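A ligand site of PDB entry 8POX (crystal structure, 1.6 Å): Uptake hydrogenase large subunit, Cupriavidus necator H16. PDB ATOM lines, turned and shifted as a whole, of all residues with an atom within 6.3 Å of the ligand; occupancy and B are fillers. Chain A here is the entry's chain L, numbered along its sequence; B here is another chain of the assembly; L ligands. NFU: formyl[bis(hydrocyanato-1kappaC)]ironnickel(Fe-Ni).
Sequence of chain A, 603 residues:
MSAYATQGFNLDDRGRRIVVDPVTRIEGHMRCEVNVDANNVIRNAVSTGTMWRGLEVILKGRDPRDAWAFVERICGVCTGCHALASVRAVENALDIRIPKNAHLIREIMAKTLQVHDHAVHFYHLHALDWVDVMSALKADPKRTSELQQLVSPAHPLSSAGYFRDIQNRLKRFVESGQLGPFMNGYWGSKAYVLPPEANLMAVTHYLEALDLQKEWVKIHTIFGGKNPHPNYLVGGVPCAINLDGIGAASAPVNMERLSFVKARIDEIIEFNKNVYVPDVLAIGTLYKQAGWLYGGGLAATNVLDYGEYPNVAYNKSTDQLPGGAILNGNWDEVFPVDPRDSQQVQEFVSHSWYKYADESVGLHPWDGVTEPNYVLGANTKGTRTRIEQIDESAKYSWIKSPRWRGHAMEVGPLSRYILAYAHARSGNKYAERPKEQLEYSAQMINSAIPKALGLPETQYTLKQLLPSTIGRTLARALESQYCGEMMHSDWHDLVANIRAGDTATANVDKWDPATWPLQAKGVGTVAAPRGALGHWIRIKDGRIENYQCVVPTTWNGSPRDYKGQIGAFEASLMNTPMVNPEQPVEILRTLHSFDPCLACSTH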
ATOM      1  N   GLU A  27      32.114  32.437  -5.524  1.00  0.00           N
ATOM      2  CA  GLU A  27      32.984  32.340  -6.687  1.00  0.00           C
ATOM      3  C   GLU A  27      32.436  33.265  -7.782  1.00  0.00           C
ATOM      4  O   GLU A  27      31.242  33.249  -8.093  1.00  0.00           O
ATOM      5  CB  GLU A  27      33.105  30.900  -7.185  1.00  0.00           C
ATOM      6  CG  GLU A  27      34.147  30.693  -8.278  1.00  0.00           C
ATOM      7  CD  GLU A  27      33.836  31.418  -9.583  1.00  0.00           C
ATOM      8  OE1 GLU A  27      32.644  31.469  -9.964  1.00  0.00           O
ATOM      9  OE2 GLU A  27      34.777  31.957 -10.221  1.00  0.00           O
ATOM     10  N   ILE A  74      35.920  26.224 -16.657  1.00  0.00           N
ATOM     11  CA  ILE A  74      34.737  26.976 -16.251  1.00  0.00           C
ATOM     12  C   ILE A  74      34.867  27.359 -14.785  1.00  0.00           C
ATOM     13  O   ILE A  74      34.464  28.451 -14.384  1.00  0.00           O
ATOM     14  CB  ILE A  74      33.433  26.167 -16.483  1.00  0.00           C
ATOM     15  CG1 ILE A  74      33.143  26.097 -17.989  1.00  0.00           C
ATOM     16  CG2 ILE A  74      32.258  26.807 -15.736  1.00  0.00           C
ATOM     17  CD1 ILE A  74      32.077  25.105 -18.373  1.00  0.00           C
ATOM     18  N   CYS A  75      35.451  26.467 -13.971  1.00  0.00           N
ATOM     19  CA  CYS A  75      35.511  26.728 -12.542  1.00  0.00           C
ATOM     20  C   CYS A  75      36.620  25.963 -11.844  1.00  0.00           C
ATOM     21  O   CYS A  75      36.712  24.747 -11.948  1.00  0.00           O
ATOM     22  CB  CYS A  75      34.184  26.378 -11.901  1.00  0.00           C
ATOM     23  SG  CYS A  75      34.091  26.827 -10.145  1.00  0.00           S
ATOM     24  N   GLY A  76      37.445  26.694 -11.099  1.00  0.00           N
ATOM     25  CA  GLY A  76      38.525  26.124 -10.302  1.00  0.00           C
ATOM     26  C   GLY A  76      38.140  25.756  -8.876  1.00  0.00           C
ATOM     27  O   GLY A  76      38.959  25.186  -8.145  1.00  0.00           O
ATOM     28  N   VAL A  77      36.922  26.108  -8.463  1.00  0.00           N
ATOM     29  CA  VAL A  77      36.376  25.720  -7.174  1.00  0.00           C
ATOM     30  C   VAL A  77      35.727  24.337  -7.299  1.00  0.00           C
ATOM     31  O   VAL A  77      36.156  23.390  -6.627  1.00  0.00           O
ATOM     32  CB  VAL A  77      35.361  26.770  -6.642  1.00  0.00           C
ATOM     33  CG1 VAL A  77      34.861  26.389  -5.254  1.00  0.00           C
ATOM     34  CG2 VAL A  77      36.016  28.144  -6.571  1.00  0.00           C
ATOM     35  N   CYS A  78      34.718  24.205  -8.167  1.00  0.00           N
ATOM     36  CA  CYS A  78      34.168  22.877  -8.475  1.00  0.00           C
ATOM     37  C   CYS A  78      35.040  22.200  -9.541  1.00  0.00           C
ATOM     38  O   CYS A  78      34.572  21.716 -10.585  1.00  0.00           O
ATOM     39  CB  CYS A  78      32.691  22.950  -8.859  1.00  0.00           C
ATOM     40  SG  CYS A  78      32.279  23.985 -10.284  1.00  0.00           S
ATOM     41  N   THR A  79      36.335  22.159  -9.235  1.00  0.00           N
ATOM     42  CA  THR A  79      37.330  21.737 -10.209  1.00  0.00           C
ATOM     43  C   THR A  79      37.251  20.244 -10.532  1.00  0.00           C
ATOM     44  O   THR A  79      37.322  19.385  -9.637  1.00  0.00           O
ATOM     45  CB  THR A  79      38.769  22.135  -9.795  1.00  0.00           C
ATOM     46  OG1 THR A  79      39.677  21.753 -10.818  1.00  0.00           O
ATOM     47  CG2 THR A  79      39.197  21.491  -8.470  1.00  0.00           C
ATOM     48  N   CYS A  81      34.512  18.689 -11.957  1.00  0.00           N
ATOM     49  CA  CYS A  81      33.151  18.208 -12.196  1.00  0.00           C
ATOM     50  C   CYS A  81      32.717  18.445 -13.646  1.00  0.00           C
ATOM     51  O   CYS A  81      32.020  17.607 -14.238  1.00  0.00           O
ATOM     52  CB  CYS A  81      32.149  18.776 -11.192  1.00  0.00           C
ATOM     53  SG  CYS A  81      31.686  20.504 -11.402  1.00  0.00           S
ATOM     54  N   HIS A  82      33.182  19.541 -14.246  1.00  0.00           N
ATOM     55  CA  HIS A  82      32.933  19.800 -15.668  1.00  0.00           C
ATOM     56  C   HIS A  82      33.716  18.845 -16.556  1.00  0.00           C
ATOM     57  O   HIS A  82      33.236  18.458 -17.614  1.00  0.00           O
ATOM     58  CB  HIS A  82      33.286  21.240 -16.022  1.00  0.00           C
ATOM     59  CG  HIS A  82      32.350  22.243 -15.445  1.00  0.00           C
ATOM     60  ND1 HIS A  82      31.052  22.397 -15.898  1.00  0.00           N
ATOM     61  CD2 HIS A  82      32.507  23.134 -14.434  1.00  0.00           C
ATOM     62  CE1 HIS A  82      30.462  23.343 -15.200  1.00  0.00           C
ATOM     63  NE2 HIS A  82      31.315  23.809 -14.303  1.00  0.00           N
ATOM     64  N   ASP A 117      35.109  21.010  -1.464  1.00  0.00           N
ATOM     65  CA  ASP A 117      34.291  22.156  -1.854  1.00  0.00           C
ATOM     66  C   ASP A 117      33.319  22.513  -0.717  1.00  0.00           C
ATOM     67  O   ASP A 117      33.238  23.671  -0.292  1.00  0.00           O
ATOM     68  CB  ASP A 117      33.535  21.816  -3.153  1.00  0.00           C
ATOM     69  CG  ASP A 117      33.164  23.028  -3.972  1.00  0.00           C
ATOM     70  OD1 ASP A 117      32.907  24.099  -3.384  1.00  0.00           O
ATOM     71  OD2 ASP A 117      33.105  22.898  -5.212  1.00  0.00           O
ATOM     72  N   ALA A 528      27.099  17.731  -9.196  1.00  0.00           N
ATOM     73  CA  ALA A 528      28.164  18.640  -8.799  1.00  0.00           C
ATOM     74  C   ALA A 528      27.895  19.183  -7.394  1.00  0.00           C
ATOM     75  O   ALA A 528      26.756  19.107  -6.913  1.00  0.00           O
ATOM     76  CB  ALA A 528      28.285  19.781  -9.789  1.00  0.00           C
ATOM     77  N   PRO A 529      28.927  19.721  -6.727  1.00  0.00           N
ATOM     78  CA  PRO A 529      28.733  20.208  -5.365  1.00  0.00           C
ATOM     79  C   PRO A 529      27.524  21.144  -5.170  1.00  0.00           C
ATOM     80  O   PRO A 529      26.876  21.073  -4.129  1.00  0.00           O
ATOM     81  CB  PRO A 529      30.048  20.921  -5.066  1.00  0.00           C
ATOM     82  CG  PRO A 529      31.046  20.144  -5.841  1.00  0.00           C
ATOM     83  CD  PRO A 529      30.335  19.778  -7.122  1.00  0.00           C
ATOM     84  N   ARG A 530      27.201  21.954  -6.172  1.00  0.00           N
ATOM     85  CA  ARG A 530      26.114  22.931  -6.060  1.00  0.00           C
ATOM     86  C   ARG A 530      24.791  22.469  -6.646  1.00  0.00           C
ATOM     87  O   ARG A 530      23.798  23.203  -6.582  1.00  0.00           O
ATOM     88  CB  ARG A 530      26.549  24.273  -6.657  1.00  0.00           C
ATOM     89  CG  ARG A 530      27.656  24.901  -5.842  1.00  0.00           C
ATOM     90  CD  ARG A 530      28.520  25.868  -6.610  1.00  0.00           C
ATOM     91  NE  ARG A 530      29.587  26.326  -5.716  1.00  0.00           N
ATOM     92  CZ  ARG A 530      30.709  25.659  -5.460  1.00  0.00           C
ATOM     93  NH1 ARG A 530      30.961  24.500  -6.049  1.00  0.00           N
ATOM     94  NH2 ARG A 530      31.586  26.171  -4.610  1.00  0.00           N
ATOM     95  N   GLY A 531      24.739  21.261  -7.207  1.00  0.00           N
ATOM     96  CA  GLY A 531      23.501  20.730  -7.741  1.00  0.00           C
ATOM     97  C   GLY A 531      23.660  19.995  -9.062  1.00  0.00           C
ATOM     98  O   GLY A 531      24.678  19.370  -9.318  1.00  0.00           O
ATOM     99  N   ALA A 532      22.634  20.095  -9.894  1.00  0.00           N
ATOM    100  CA  ALA A 532      22.509  19.319 -11.126  1.00  0.00           C
ATOM    101  C   ALA A 532      23.322  19.934 -12.264  1.00  0.00           C
ATOM    102  O   ALA A 532      23.017  21.048 -12.713  1.00  0.00           O
ATOM    103  CB  ALA A 532      21.035  19.218 -11.506  1.00  0.00           C
ATOM    104  N   LEU A 533      24.324  19.203 -12.730  1.00  0.00           N
ATOM    105  CA  LEU A 533      25.173  19.619 -13.859  1.00  0.00           C
ATOM    106  C   LEU A 533      24.940  18.731 -15.073  1.00  0.00           C
ATOM    107  O   LEU A 533      24.925  17.509 -14.954  1.00  0.00           O
ATOM    108  CB  LEU A 533      26.654  19.536 -13.464  1.00  0.00           C
ATOM    109  CG  LEU A 533      27.668  19.779 -14.594  1.00  0.00           C
ATOM    110  CD1 LEU A 533      27.560  21.191 -15.175  1.00  0.00           C
ATOM    111  CD2 LEU A 533      29.080  19.529 -14.097  1.00  0.00           C
ATOM    112  N   VAL A 551      24.382  24.468 -15.719  1.00  0.00           N
ATOM    113  CA  VAL A 551      25.217  24.290 -14.534  1.00  0.00           C
ATOM    114  C   VAL A 551      24.364  24.584 -13.280  1.00  0.00           C
ATOM    115  O   VAL A 551      23.348  25.289 -13.379  1.00  0.00           O
ATOM    116  CB  VAL A 551      26.459  25.200 -14.692  1.00  0.00           C
ATOM    117  CG1 VAL A 551      27.482  24.972 -13.612  1.00  0.00           C
ATOM    118  CG2 VAL A 551      27.102  24.965 -16.048  1.00  0.00           C
ATOM    119  N   PRO A 552      24.726  24.037 -12.092  1.00  0.00           N
ATOM    120  CA  PRO A 552      23.817  24.192 -10.960  1.00  0.00           C
ATOM    121  C   PRO A 552      23.459  25.635 -10.638  1.00  0.00           C
ATOM    122  O   PRO A 552      22.294  25.945 -10.399  1.00  0.00           O
ATOM    123  CB  PRO A 552      24.592  23.548  -9.800  1.00  0.00           C
ATOM    124  CG  PRO A 552      25.444  22.518 -10.450  1.00  0.00           C
ATOM    125  CD  PRO A 552      25.835  23.102 -11.772  1.00  0.00           C
ATOM    126  N   THR A 553      24.447  26.523 -10.630  1.00  0.00           N
ATOM    127  CA  THR A 553      24.186  27.920 -10.300  1.00  0.00           C
ATOM    128  C   THR A 553      23.448  28.612 -11.450  1.00  0.00           C
ATOM    129  O   THR A 553      22.795  29.641 -11.221  1.00  0.00           O
ATOM    130  CB  THR A 553      25.461  28.658  -9.848  1.00  0.00           C
ATOM    131  OG1 THR A 553      26.043  27.955  -8.747  1.00  0.00           O
ATOM    132  CG2 THR A 553      25.121  30.084  -9.386  1.00  0.00           C
ATOM    133  N   THR A 554      23.476  28.033 -12.657  1.00  0.00           N
ATOM    134  CA  THR A 554      22.584  28.519 -13.727  1.00  0.00           C
ATOM    135  C   THR A 554      21.144  28.326 -13.275  1.00  0.00           C
ATOM    136  O   THR A 554      20.338  29.265 -13.388  1.00  0.00           O
ATOM    137  CB  THR A 554      22.798  27.792 -15.083  1.00  0.00           C
ATOM    138  OG1 THR A 554      24.198  27.682 -15.379  1.00  0.00           O
ATOM    139  CG2 THR A 554      22.087  28.537 -16.213  1.00  0.00           C
ATOM    140  N   ASP A 595      25.780  28.423  -2.029  1.00  0.00           N
ATOM    141  CA  ASP A 595      27.158  28.300  -2.462  1.00  0.00           C
ATOM    142  C   ASP A 595      27.265  28.764  -3.926  1.00  0.00           C
ATOM    143  O   ASP A 595      27.632  27.983  -4.813  1.00  0.00           O
ATOM    144  CB  ASP A 595      27.584  26.837  -2.268  1.00  0.00           C
ATOM    145  CG  ASP A 595      29.019  26.552  -2.625  1.00  0.00           C
ATOM    146  OD1 ASP A 595      29.834  27.487  -2.828  1.00  0.00           O
ATOM    147  OD2 ASP A 595      29.312  25.346  -2.711  1.00  0.00           O
ATOM    148  N   PRO A 596      26.927  30.033  -4.191  1.00  0.00           N
ATOM    149  CA  PRO A 596      26.858  30.473  -5.583  1.00  0.00           C
ATOM    150  C   PRO A 596      28.201  30.400  -6.303  1.00  0.00           C
ATOM    151  O   PRO A 596      29.219  30.863  -5.785  1.00  0.00           O
ATOM    152  CB  PRO A 596      26.396  31.934  -5.469  1.00  0.00           C
ATOM    153  CG  PRO A 596      25.724  32.017  -4.145  1.00  0.00           C
ATOM    154  CD  PRO A 596      26.558  31.127  -3.278  1.00  0.00           C
ATOM    155  N   CYS A 597      28.195  29.777  -7.477  1.00  0.00           N
ATOM    156  CA  CYS A 597      29.379  29.741  -8.331  1.00  0.00           C
ATOM    157  C   CYS A 597      29.059  30.458  -9.630  1.00  0.00           C
ATOM    158  O   CYS A 597      28.437  29.893 -10.534  1.00  0.00           O
ATOM    159  CB  CYS A 597      29.815  28.319  -8.584  1.00  0.00           C
ATOM    160  SG  CYS A 597      31.466  28.216  -9.305  1.00  0.00           S
ATOM    161  N   LEU A 598      29.466  31.717  -9.721  1.00  0.00           N
ATOM    162  CA  LEU A 598      28.990  32.573 -10.800  1.00  0.00           C
ATOM    163  C   LEU A 598      29.691  32.311 -12.133  1.00  0.00           C
ATOM    164  O   LEU A 598      29.063  32.401 -13.182  1.00  0.00           O
ATOM    165  CB  LEU A 598      29.063  34.050 -10.407  1.00  0.00           C
ATOM    166  CG  LEU A 598      27.851  34.537  -9.589  1.00  0.00           C
ATOM    167  CD1 LEU A 598      26.608  34.653 -10.460  1.00  0.00           C
ATOM    168  CD2 LEU A 598      27.567  33.665  -8.374  1.00  0.00           C
ATOM    169  N   ALA A 599      30.974  31.959 -12.091  1.00  0.00           N
ATOM    170  CA  ALA A 599      31.697  31.575 -13.297  1.00  0.00           C
ATOM    171  C   ALA A 599      31.080  30.307 -13.877  1.00  0.00           C
ATOM    172  O   ALA A 599      30.918  30.179 -15.092  1.00  0.00           O
ATOM    173  CB  ALA A 599      33.167  31.368 -12.997  1.00  0.00           C
ATOM    174  N   CYS A 600      30.719  29.375 -13.007  1.00  0.00           N
ATOM    175  CA  CYS A 600      29.954  28.197 -13.407  1.00  0.00           C
ATOM    176  C   CYS A 600      28.628  28.575 -14.053  1.00  0.00           C
ATOM    177  O   CYS A 600      28.274  28.058 -15.113  1.00  0.00           O
ATOM    178  CB  CYS A 600      29.650  27.320 -12.200  1.00  0.00           C
ATOM    179  SG  CYS A 600      30.749  25.905 -12.032  1.00  0.00           S
ATOM    180  N   SER A 601      27.917  29.501 -13.427  1.00  0.00           N
ATOM    181  CA  SER A 601      26.546  29.793 -13.849  1.00  0.00           C
ATOM    182  C   SER A 601      26.500  30.349 -15.273  1.00  0.00           C
ATOM    183  O   SER A 601      25.529  30.110 -15.984  1.00  0.00           O
ATOM    184  CB  SER A 601      25.888  30.773 -12.876  1.00  0.00           C
ATOM    185  OG  SER A 601      26.385  32.085 -13.014  1.00  0.00           O
ATOM    186  N   CYS B  17      38.264  31.662 -13.377  1.00  0.00           N
ATOM    187  CA  CYS B  17      37.584  30.488 -12.815  1.00  0.00           C
ATOM    188  C   CYS B  17      37.803  30.341 -11.313  1.00  0.00           C
ATOM    189  O   CYS B  17      37.236  29.438 -10.699  1.00  0.00           O
ATOM    190  CB  CYS B  17      38.039  29.223 -13.548  1.00  0.00           C
ATOM    191  SG  CYS B  17      39.545  28.466 -12.924  1.00  0.00           S
HETATM  192 FE   NFU L   1      30.009  24.472 -10.340  1.00  0.00          FE
HETATM  193 NI   NFU L   1      31.984  26.179  -9.755  1.00  0.00          NI
HETATM  194  C1  NFU L   1      29.543  23.385  -8.971  1.00  0.00           C
HETATM  195  N1  NFU L   1      29.267  22.710  -8.083  1.00  0.00           N
HETATM  196  C2  NFU L   1      28.361  25.285 -10.206  1.00  0.00           C
HETATM  197  N2  NFU L   1      27.352  25.815 -10.107  1.00  0.00           N
HETATM  198  C3  NFU L   1      29.364  23.153 -11.440  1.00  0.00           C
HETATM  199  O3  NFU L   1      28.945  22.364 -12.122  1.00  0.00           O
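The side-chain sulfur (SG) of Cys 78 is bound to a nickel atom (NI) of the ligand. The side-chain sulfur of Cys 75 is bound to a nickel atom (NI) of the ligand (2.2 Å). SG of Cys 600 binds FE of the ligand. NH1 of Arg 530 sits at hydrogen-bond distance from N1 of the ligand (3.2 Å). The side-chain sulfur (SG) of Cys 81 sits at hydrogen-bond distance from an oxygen (O3) of the ligand (3.4 Å). NI of the ligand is bound by SG of Cys 597. The backbone NH (N) of Arg 530 lies within hydrogen-bond range of a nitrogen (N1) of the ligand (2.9 Å). A nitrogen (N2) of the ligand sits at hydrogen-bond distance from the side-chain hydroxyl (OG1) of Thr 553, 2.9 Å away. A nitrogen (N2) of the ligand is in hydrogen-bond range of the backbone NH of Thr 553.
The side-chain sulfur of Cys 600 lies close to a ring nitrogen (NE2) of His 82. The backbone carbonyl oxygen of Val 551 lies close to the side-chain hydroxyl of Thr 554, at 3.2 Å. The guanidinium group of Arg 530 is in salt-bridge range of the side-chain carboxylate of Asp 117. NH2 of Arg 530 lies within salt-bridge range of OD1 of Asp 595, 2.8 Å away. The backbone carbonyl oxygen (O) of Cys 78 lies within hydrogen-bond range of the side-chain sulfur (SG) of Cys 81 (3.2 Å). The backbone NH (N) of Cys 597 sits at hydrogen-bond distance from the side-chain hydroxyl (OG1) of Thr 553. The side-chain sulfur (SG) of Cys 597 lies close to the side-chain carboxylate (OE1) of Glu 27 (3.5 Å). SG of Cys 75 sits close to N of Val 77.
A nitrogen (N1) of the ligand lies close to the backbone nitrogen (N) of Pro 529 (3.3 Å). Merely in contact with the ligand: His 82 (3.5 Å), Ala 528 (3.5 Å), Leu 533 (3.5 Å), Val 551 (3.3 Å) and Pro 552 (3.2 Å). Hydrophobic or aromatic side chains within 4 Å of the ligand: His 82, Ala 528, Pro 529, Leu 533, Val 551 and Pro 552.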
